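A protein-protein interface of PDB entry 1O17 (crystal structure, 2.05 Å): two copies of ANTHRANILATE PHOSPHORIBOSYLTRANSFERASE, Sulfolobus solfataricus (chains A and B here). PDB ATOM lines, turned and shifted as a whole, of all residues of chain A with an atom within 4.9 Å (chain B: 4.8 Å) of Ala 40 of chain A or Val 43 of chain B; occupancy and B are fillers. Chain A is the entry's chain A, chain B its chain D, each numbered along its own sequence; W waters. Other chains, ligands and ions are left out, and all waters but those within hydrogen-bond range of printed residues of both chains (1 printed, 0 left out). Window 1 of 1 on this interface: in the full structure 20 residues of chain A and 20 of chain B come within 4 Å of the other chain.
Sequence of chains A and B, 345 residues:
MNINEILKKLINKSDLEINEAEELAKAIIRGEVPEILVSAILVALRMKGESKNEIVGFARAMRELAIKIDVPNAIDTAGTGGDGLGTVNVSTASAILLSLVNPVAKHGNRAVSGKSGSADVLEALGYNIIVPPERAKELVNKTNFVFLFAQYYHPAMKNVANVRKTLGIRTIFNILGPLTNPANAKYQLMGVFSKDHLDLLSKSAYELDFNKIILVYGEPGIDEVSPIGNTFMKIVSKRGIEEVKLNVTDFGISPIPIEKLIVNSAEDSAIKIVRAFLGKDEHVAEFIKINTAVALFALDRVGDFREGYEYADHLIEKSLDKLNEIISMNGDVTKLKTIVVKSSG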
ATOM      1  N   LEU A   7      17.985 -10.237 -22.974  1.00  0.00           N
ATOM      2  CA  LEU A   7      17.025 -10.010 -24.052  1.00  0.00           C
ATOM      3  C   LEU A   7      17.672  -9.347 -25.261  1.00  0.00           C
ATOM      4  O   LEU A   7      17.507  -9.808 -26.392  1.00  0.00           O
ATOM      5  CB  LEU A   7      15.854  -9.155 -23.557  1.00  0.00           C
ATOM      6  CG  LEU A   7      14.768  -8.813 -24.591  1.00  0.00           C
ATOM      7  CD1 LEU A   7      14.235 -10.077 -25.256  1.00  0.00           C
ATOM      8  CD2 LEU A   7      13.643  -8.063 -23.897  1.00  0.00           C
ATOM      9  N   ILE A  11      17.618 -10.711 -29.054  1.00  0.00           N
ATOM     10  CA  ILE A  11      17.044  -9.848 -30.082  1.00  0.00           C
ATOM     11  C   ILE A  11      18.036  -9.695 -31.229  1.00  0.00           C
ATOM     12  O   ILE A  11      17.650  -9.486 -32.375  1.00  0.00           O
ATOM     13  CB  ILE A  11      16.727  -8.447 -29.521  1.00  0.00           C
ATOM     14  CG1 ILE A  11      15.608  -8.540 -28.484  1.00  0.00           C
ATOM     15  CG2 ILE A  11      16.331  -7.515 -30.644  1.00  0.00           C
ATOM     16  CD1 ILE A  11      14.294  -9.052 -29.043  1.00  0.00           C
ATOM     17  N   GLU A  35       6.203 -11.162 -16.260  1.00  0.00           N
ATOM     18  CA  GLU A  35       5.597 -11.907 -17.369  1.00  0.00           C
ATOM     19  C   GLU A  35       5.904 -11.284 -18.734  1.00  0.00           C
ATOM     20  O   GLU A  35       6.167 -11.997 -19.704  1.00  0.00           O
ATOM     21  CB  GLU A  35       4.079 -12.010 -17.182  1.00  0.00           C
ATOM     22  CG  GLU A  35       3.660 -12.768 -15.922  1.00  0.00           C
ATOM     23  CD  GLU A  35       2.176 -13.107 -15.916  1.00  0.00           C
ATOM     24  OE1 GLU A  35       1.368 -12.263 -16.351  1.00  0.00           O
ATOM     25  OE2 GLU A  35       1.816 -14.216 -15.469  1.00  0.00           O
ATOM     26  N   ILE A  36       5.874  -9.954 -18.802  1.00  0.00           N
ATOM     27  CA  ILE A  36       6.163  -9.239 -20.043  1.00  0.00           C
ATOM     28  C   ILE A  36       7.542  -9.626 -20.569  1.00  0.00           C
ATOM     29  O   ILE A  36       7.720  -9.805 -21.774  1.00  0.00           O
ATOM     30  CB  ILE A  36       6.101  -7.714 -19.822  1.00  0.00           C
ATOM     31  CG1 ILE A  36       4.641  -7.280 -19.682  1.00  0.00           C
ATOM     32  CG2 ILE A  36       6.772  -6.964 -20.981  1.00  0.00           C
ATOM     33  CD1 ILE A  36       4.473  -5.866 -19.162  1.00  0.00           C
ATOM     34  N   LEU A  37       8.508  -9.766 -19.663  1.00  0.00           N
ATOM     35  CA  LEU A  37       9.872 -10.129 -20.045  1.00  0.00           C
ATOM     36  C   LEU A  37      10.023 -11.636 -20.303  1.00  0.00           C
ATOM     37  O   LEU A  37      10.830 -12.043 -21.137  1.00  0.00           O
ATOM     38  CB  LEU A  37      10.873  -9.653 -18.973  1.00  0.00           C
ATOM     39  CG  LEU A  37      11.153  -8.137 -18.932  1.00  0.00           C
ATOM     40  CD1 LEU A  37      12.050  -7.789 -17.754  1.00  0.00           C
ATOM     41  CD2 LEU A  37      11.824  -7.704 -20.224  1.00  0.00           C
ATOM     42  N   VAL A  38       9.255 -12.465 -19.596  1.00  0.00           N
ATOM     43  CA  VAL A  38       9.326 -13.911 -19.834  1.00  0.00           C
ATOM     44  C   VAL A  38       8.801 -14.164 -21.249  1.00  0.00           C
ATOM     45  O   VAL A  38       9.378 -14.933 -22.014  1.00  0.00           O
ATOM     46  CB  VAL A  38       8.461 -14.723 -18.822  1.00  0.00           C
ATOM     47  CG1 VAL A  38       8.478 -16.205 -19.204  1.00  0.00           C
ATOM     48  CG2 VAL A  38       8.997 -14.550 -17.398  1.00  0.00           C
ATOM     49  N   SER A  39       7.700 -13.501 -21.590  1.00  0.00           N
ATOM     50  CA  SER A  39       7.090 -13.626 -22.911  1.00  0.00           C
ATOM     51  C   SER A  39       8.093 -13.203 -23.987  1.00  0.00           C
ATOM     52  O   SER A  39       8.300 -13.916 -24.977  1.00  0.00           O
ATOM     53  CB  SER A  39       5.837 -12.745 -22.982  1.00  0.00           C
ATOM     54  OG  SER A  39       5.225 -12.820 -24.259  1.00  0.00           O
ATOM     55  N   ALA A  40       8.726 -12.046 -23.784  1.00  0.00           N
ATOM     56  CA  ALA A  40       9.711 -11.538 -24.739  1.00  0.00           C
ATOM     57  C   ALA A  40      10.835 -12.534 -24.951  1.00  0.00           C
ATOM     58  O   ALA A  40      11.227 -12.816 -26.080  1.00  0.00           O
ATOM     59  CB  ALA A  40      10.296 -10.200 -24.249  1.00  0.00           C
ATOM     60  N   ILE A  41      11.354 -13.064 -23.855  1.00  0.00           N
ATOM     61  CA  ILE A  41      12.454 -14.014 -23.900  1.00  0.00           C
ATOM     62  C   ILE A  41      12.120 -15.320 -24.627  1.00  0.00           C
ATOM     63  O   ILE A  41      12.932 -15.831 -25.403  1.00  0.00           O
ATOM     64  CB  ILE A  41      12.949 -14.309 -22.469  1.00  0.00           C
ATOM     65  CG1 ILE A  41      13.667 -13.069 -21.926  1.00  0.00           C
ATOM     66  CG2 ILE A  41      13.881 -15.520 -22.460  1.00  0.00           C
ATOM     67  CD1 ILE A  41      14.132 -13.200 -20.499  1.00  0.00           C
ATOM     68  N   LEU A  42      10.931 -15.856 -24.391  1.00  0.00           N
ATOM     69  CA  LEU A  42      10.538 -17.095 -25.046  1.00  0.00           C
ATOM     70  C   LEU A  42      10.327 -16.880 -26.543  1.00  0.00           C
ATOM     71  O   LEU A  42      10.664 -17.739 -27.352  1.00  0.00           O
ATOM     72  CB  LEU A  42       9.275 -17.664 -24.391  1.00  0.00           C
ATOM     73  CG  LEU A  42       9.491 -18.124 -22.944  1.00  0.00           C
ATOM     74  CD1 LEU A  42       8.230 -18.796 -22.416  1.00  0.00           C
ATOM     75  CD2 LEU A  42      10.669 -19.089 -22.885  1.00  0.00           C
ATOM     76  N   VAL A  43       9.795 -15.722 -26.915  1.00  0.00           N
ATOM     77  CA  VAL A  43       9.571 -15.435 -28.319  1.00  0.00           C
ATOM     78  C   VAL A  43      10.908 -15.197 -29.029  1.00  0.00           C
ATOM     79  O   VAL A  43      11.115 -15.668 -30.153  1.00  0.00           O
ATOM     80  CB  VAL A  43       8.642 -14.212 -28.486  1.00  0.00           C
ATOM     81  CG1 VAL A  43       8.535 -13.814 -29.971  1.00  0.00           C
ATOM     82  CG2 VAL A  43       7.257 -14.551 -27.940  1.00  0.00           C
ATOM     83  N   ALA A  44      11.821 -14.490 -28.369  1.00  0.00           N
ATOM     84  CA  ALA A  44      13.138 -14.200 -28.954  1.00  0.00           C
ATOM     85  C   ALA A  44      13.928 -15.491 -29.194  1.00  0.00           C
ATOM     86  O   ALA A  44      14.567 -15.652 -30.230  1.00  0.00           O
ATOM     87  CB  ALA A  44      13.929 -13.260 -28.028  1.00  0.00           C
ATOM     88  N   SER B  39       3.781  -7.782 -25.784  1.00  0.00           N
ATOM     89  CA  SER B  39       5.224  -7.983 -25.683  1.00  0.00           C
ATOM     90  C   SER B  39       5.714  -8.961 -26.753  1.00  0.00           C
ATOM     91  O   SER B  39       6.707  -8.704 -27.441  1.00  0.00           O
ATOM     92  CB  SER B  39       5.586  -8.517 -24.295  1.00  0.00           C
ATOM     93  OG  SER B  39       6.971  -8.801 -24.203  1.00  0.00           O
ATOM     94  N   ALA B  40       5.004 -10.077 -26.897  1.00  0.00           N
ATOM     95  CA  ALA B  40       5.381 -11.087 -27.873  1.00  0.00           C
ATOM     96  C   ALA B  40       5.349 -10.541 -29.299  1.00  0.00           C
ATOM     97  O   ALA B  40       6.263 -10.795 -30.084  1.00  0.00           O
ATOM     98  CB  ALA B  40       4.461 -12.304 -27.752  1.00  0.00           C
ATOM     99  N   ILE B  41       4.290  -9.802 -29.624  1.00  0.00           N
ATOM    100  CA  ILE B  41       4.125  -9.228 -30.954  1.00  0.00           C
ATOM    101  C   ILE B  41       5.206  -8.198 -31.291  1.00  0.00           C
ATOM    102  O   ILE B  41       5.737  -8.203 -32.401  1.00  0.00           O
ATOM    103  CB  ILE B  41       2.713  -8.593 -31.108  1.00  0.00           C
ATOM    104  CG1 ILE B  41       1.659  -9.699 -31.232  1.00  0.00           C
ATOM    105  CG2 ILE B  41       2.661  -7.699 -32.331  1.00  0.00           C
ATOM    106  CD1 ILE B  41       0.239  -9.185 -31.342  1.00  0.00           C
ATOM    107  N   LEU B  42       5.533  -7.326 -30.342  1.00  0.00           N
ATOM    108  CA  LEU B  42       6.564  -6.306 -30.559  1.00  0.00           C
ATOM    109  C   LEU B  42       7.937  -6.957 -30.755  1.00  0.00           C
ATOM    110  O   LEU B  42       8.719  -6.525 -31.600  1.00  0.00           O
ATOM    111  CB  LEU B  42       6.608  -5.324 -29.374  1.00  0.00           C
ATOM    112  CG  LEU B  42       5.333  -4.486 -29.149  1.00  0.00           C
ATOM    113  CD1 LEU B  42       5.535  -3.474 -27.997  1.00  0.00           C
ATOM    114  CD2 LEU B  42       4.985  -3.746 -30.439  1.00  0.00           C
ATOM    115  N   VAL B  43       8.220  -8.002 -29.978  1.00  0.00           N
ATOM    116  CA  VAL B  43       9.493  -8.710 -30.083  1.00  0.00           C
ATOM    117  C   VAL B  43       9.545  -9.437 -31.423  1.00  0.00           C
ATOM    118  O   VAL B  43      10.550  -9.373 -32.140  1.00  0.00           O
ATOM    119  CB  VAL B  43       9.666  -9.723 -28.922  1.00  0.00           C
ATOM    120  CG1 VAL B  43      10.786 -10.701 -29.222  1.00  0.00           C
ATOM    121  CG2 VAL B  43       9.963  -8.971 -27.625  1.00  0.00           C
ATOM    122  N   ALA B  44       8.440 -10.100 -31.765  1.00  0.00           N
ATOM    123  CA  ALA B  44       8.332 -10.846 -33.017  1.00  0.00           C
ATOM    124  C   ALA B  44       8.517  -9.929 -34.229  1.00  0.00           C
ATOM    125  O   ALA B  44       9.231 -10.280 -35.172  1.00  0.00           O
ATOM    126  CB  ALA B  44       6.970 -11.559 -33.087  1.00  0.00           C
ATOM    127  N   LEU B  45       7.870  -8.763 -34.201  1.00  0.00           N
ATOM    128  CA  LEU B  45       7.977  -7.786 -35.293  1.00  0.00           C
ATOM    129  C   LEU B  45       9.437  -7.385 -35.491  1.00  0.00           C
ATOM    130  O   LEU B  45       9.973  -7.420 -36.602  1.00  0.00           O
ATOM    131  CB  LEU B  45       7.187  -6.512 -34.975  1.00  0.00           C
ATOM    132  CG  LEU B  45       5.834  -6.114 -35.576  1.00  0.00           C
ATOM    133  CD1 LEU B  45       5.509  -6.937 -36.814  1.00  0.00           C
ATOM    134  CD2 LEU B  45       4.759  -6.246 -34.522  1.00  0.00           C
ATOM    135  N   ARG B  46      10.082  -6.989 -34.404  1.00  0.00           N
ATOM    136  CA  ARG B  46      11.466  -6.570 -34.499  1.00  0.00           C
ATOM    137  C   ARG B  46      12.399  -7.654 -35.035  1.00  0.00           C
ATOM    138  O   ARG B  46      13.233  -7.392 -35.904  1.00  0.00           O
ATOM    139  CB  ARG B  46      11.970  -6.087 -33.146  1.00  0.00           C
ATOM    140  CG  ARG B  46      13.437  -5.715 -33.216  1.00  0.00           C
ATOM    141  CD  ARG B  46      13.909  -4.922 -32.030  1.00  0.00           C
ATOM    142  NE  ARG B  46      15.351  -4.736 -32.123  1.00  0.00           N
ATOM    143  CZ  ARG B  46      16.080  -4.072 -31.236  1.00  0.00           C
ATOM    144  NH1 ARG B  46      15.508  -3.514 -30.175  1.00  0.00           N
ATOM    145  NH2 ARG B  46      17.388  -3.983 -31.410  1.00  0.00           N
ATOM    146  N   MET B  47      12.257  -8.874 -34.532  1.00  0.00           N
ATOM    147  CA  MET B  47      13.127  -9.951 -34.981  1.00  0.00           C
ATOM    148  C   MET B  47      12.850 -10.397 -36.401  1.00  0.00           C
ATOM    149  O   MET B  47      13.757 -10.833 -37.104  1.00  0.00           O
ATOM    150  CB  MET B  47      13.046 -11.109 -34.007  1.00  0.00           C
ATOM    151  CG  MET B  47      13.589 -10.687 -32.672  1.00  0.00           C
ATOM    152  SD  MET B  47      13.920 -12.031 -31.612  1.00  0.00           S
ATOM    153  CE  MET B  47      15.368 -12.772 -32.390  1.00  0.00           C
ATOM    154  N   LEU B 167       9.870  -3.834 -21.259  1.00  0.00           N
ATOM    155  CA  LEU B 167      10.691  -4.448 -22.296  1.00  0.00           C
ATOM    156  C   LEU B 167      12.086  -3.835 -22.309  1.00  0.00           C
ATOM    157  O   LEU B 167      13.086  -4.552 -22.360  1.00  0.00           O
ATOM    158  CB  LEU B 167      10.052  -4.259 -23.670  1.00  0.00           C
ATOM    159  CG  LEU B 167       9.039  -5.317 -24.114  1.00  0.00           C
ATOM    160  CD1 LEU B 167       8.501  -4.947 -25.487  1.00  0.00           C
ATOM    161  CD2 LEU B 167       9.713  -6.683 -24.159  1.00  0.00           C
ATOM    162  N   ILE B 169      13.597  -2.235 -24.659  1.00  0.00           N
ATOM    163  CA  ILE B 169      14.285  -2.355 -25.939  1.00  0.00           C
ATOM    164  C   ILE B 169      13.472  -1.566 -26.954  1.00  0.00           C
ATOM    165  O   ILE B 169      12.264  -1.377 -26.777  1.00  0.00           O
ATOM    166  CB  ILE B 169      14.381  -3.824 -26.445  1.00  0.00           C
ATOM    167  CG1 ILE B 169      12.977  -4.407 -26.635  1.00  0.00           C
ATOM    168  CG2 ILE B 169      15.210  -4.659 -25.483  1.00  0.00           C
ATOM    169  CD1 ILE B 169      12.943  -5.754 -27.348  1.00  0.00           C
HETATM  170  O   HOH W   1      16.427  -7.709 -34.594  1.00  0.00           O
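O of Ile 36 of chain A is in hydrogen-bond range of OG of Ser 39 of chain B.
Among the printed residues, merely in contact across the chains: Ile 11 of chain A with Arg 46 of chain B, Ala 44 of chain A with Met 47 of chain B, Ala 40 of chain A with Leu 167 of chain B, Val 43 of chain A with Ala 40 of chain B, Ala 40 of chain A with Ser 39 of chain B, Ala 40 of chain A with Val 43 of chain B, Ser 39 of chain A with Ala 40 of chain B, Leu 7 of chain A with Leu 167 of chain B, Ile 11 of chain A with Val 43 of chain B, Val 43 of chain A with Val 43 of chain B, Ile 11 of chain A with Ile 169 of chain B and Ile 11 of chain A with Met 47 of chain B.
Printed residues of chain A within 4 Å of Val 43 of chain B: Ile 11, Ala 40 and Val 43.
Of the printed residues of chain A, Leu 167 of chain B touches Leu 7 (3.9 Å) and Ala 40 (3.6 Å).
Printed residues of chain B within 4 Å of Leu 7 of chain A: Leu 167 (3.9 Å).
Ile 41 of chain A touches none of the printed residues of chain B.
The nearest printed residue of chain B that does not touch Ala 40 of chain A is Ala 40 of chain B (5.2 Å).
The nearest printed residue of chain A that does not touch Val 43 of chain B is Ala 44 of chain A (4.02 Å).
Printed residues of chain A that touch a printed residue of chain B: Leu 7, Ile 11, Ile 36, Ser 39, Ala 40, Val 43 and Ala 44.
Hydrophobic or aromatic side chains of chain A within 4 Å of the printed part of chain B: Leu 7, Ile 11, Ile 36, Ala 40, Val 43 and Ala 44.
Hydrophobic or aromatic side chains of chain B within 4 Å of the printed part of chain A: Ala 40, Val 43, Met 47, Leu 167 and Ile 169.
Along chain B the printed residues that touch a printed residue of chain A span positions 39 to 169.
Among the printed residues, no Asp or Glu carboxylate lies within 4 Å of a Lys or Arg side-chain nitrogen of the other chain.
Ser 39 of chain A touches Ala 40 of chain B, and with the chains exchanged Ala 40 of chain A touches Ser 39 of chain B.
Ala 40 of chain A touches Val 43 of chain B, and with the chains exchanged Val 43 of chain A touches Ala 40 of chain B.
Val 43 of chain B touches its own counterpart, Val 43 of chain A.
Positions printed for both chains: 39, 40, 41, 42, 43 and 44.
Of the 13 pairs that touch across the chains among the printed residues, 5 have their exchanged pair printed and touching as well.
Water W1 bridges the backbone carbonyl oxygen of Ile 11 of chain A (3.1 Å) and the backbone carbonyl oxygen of Arg 46 of chain B (3.5 Å).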
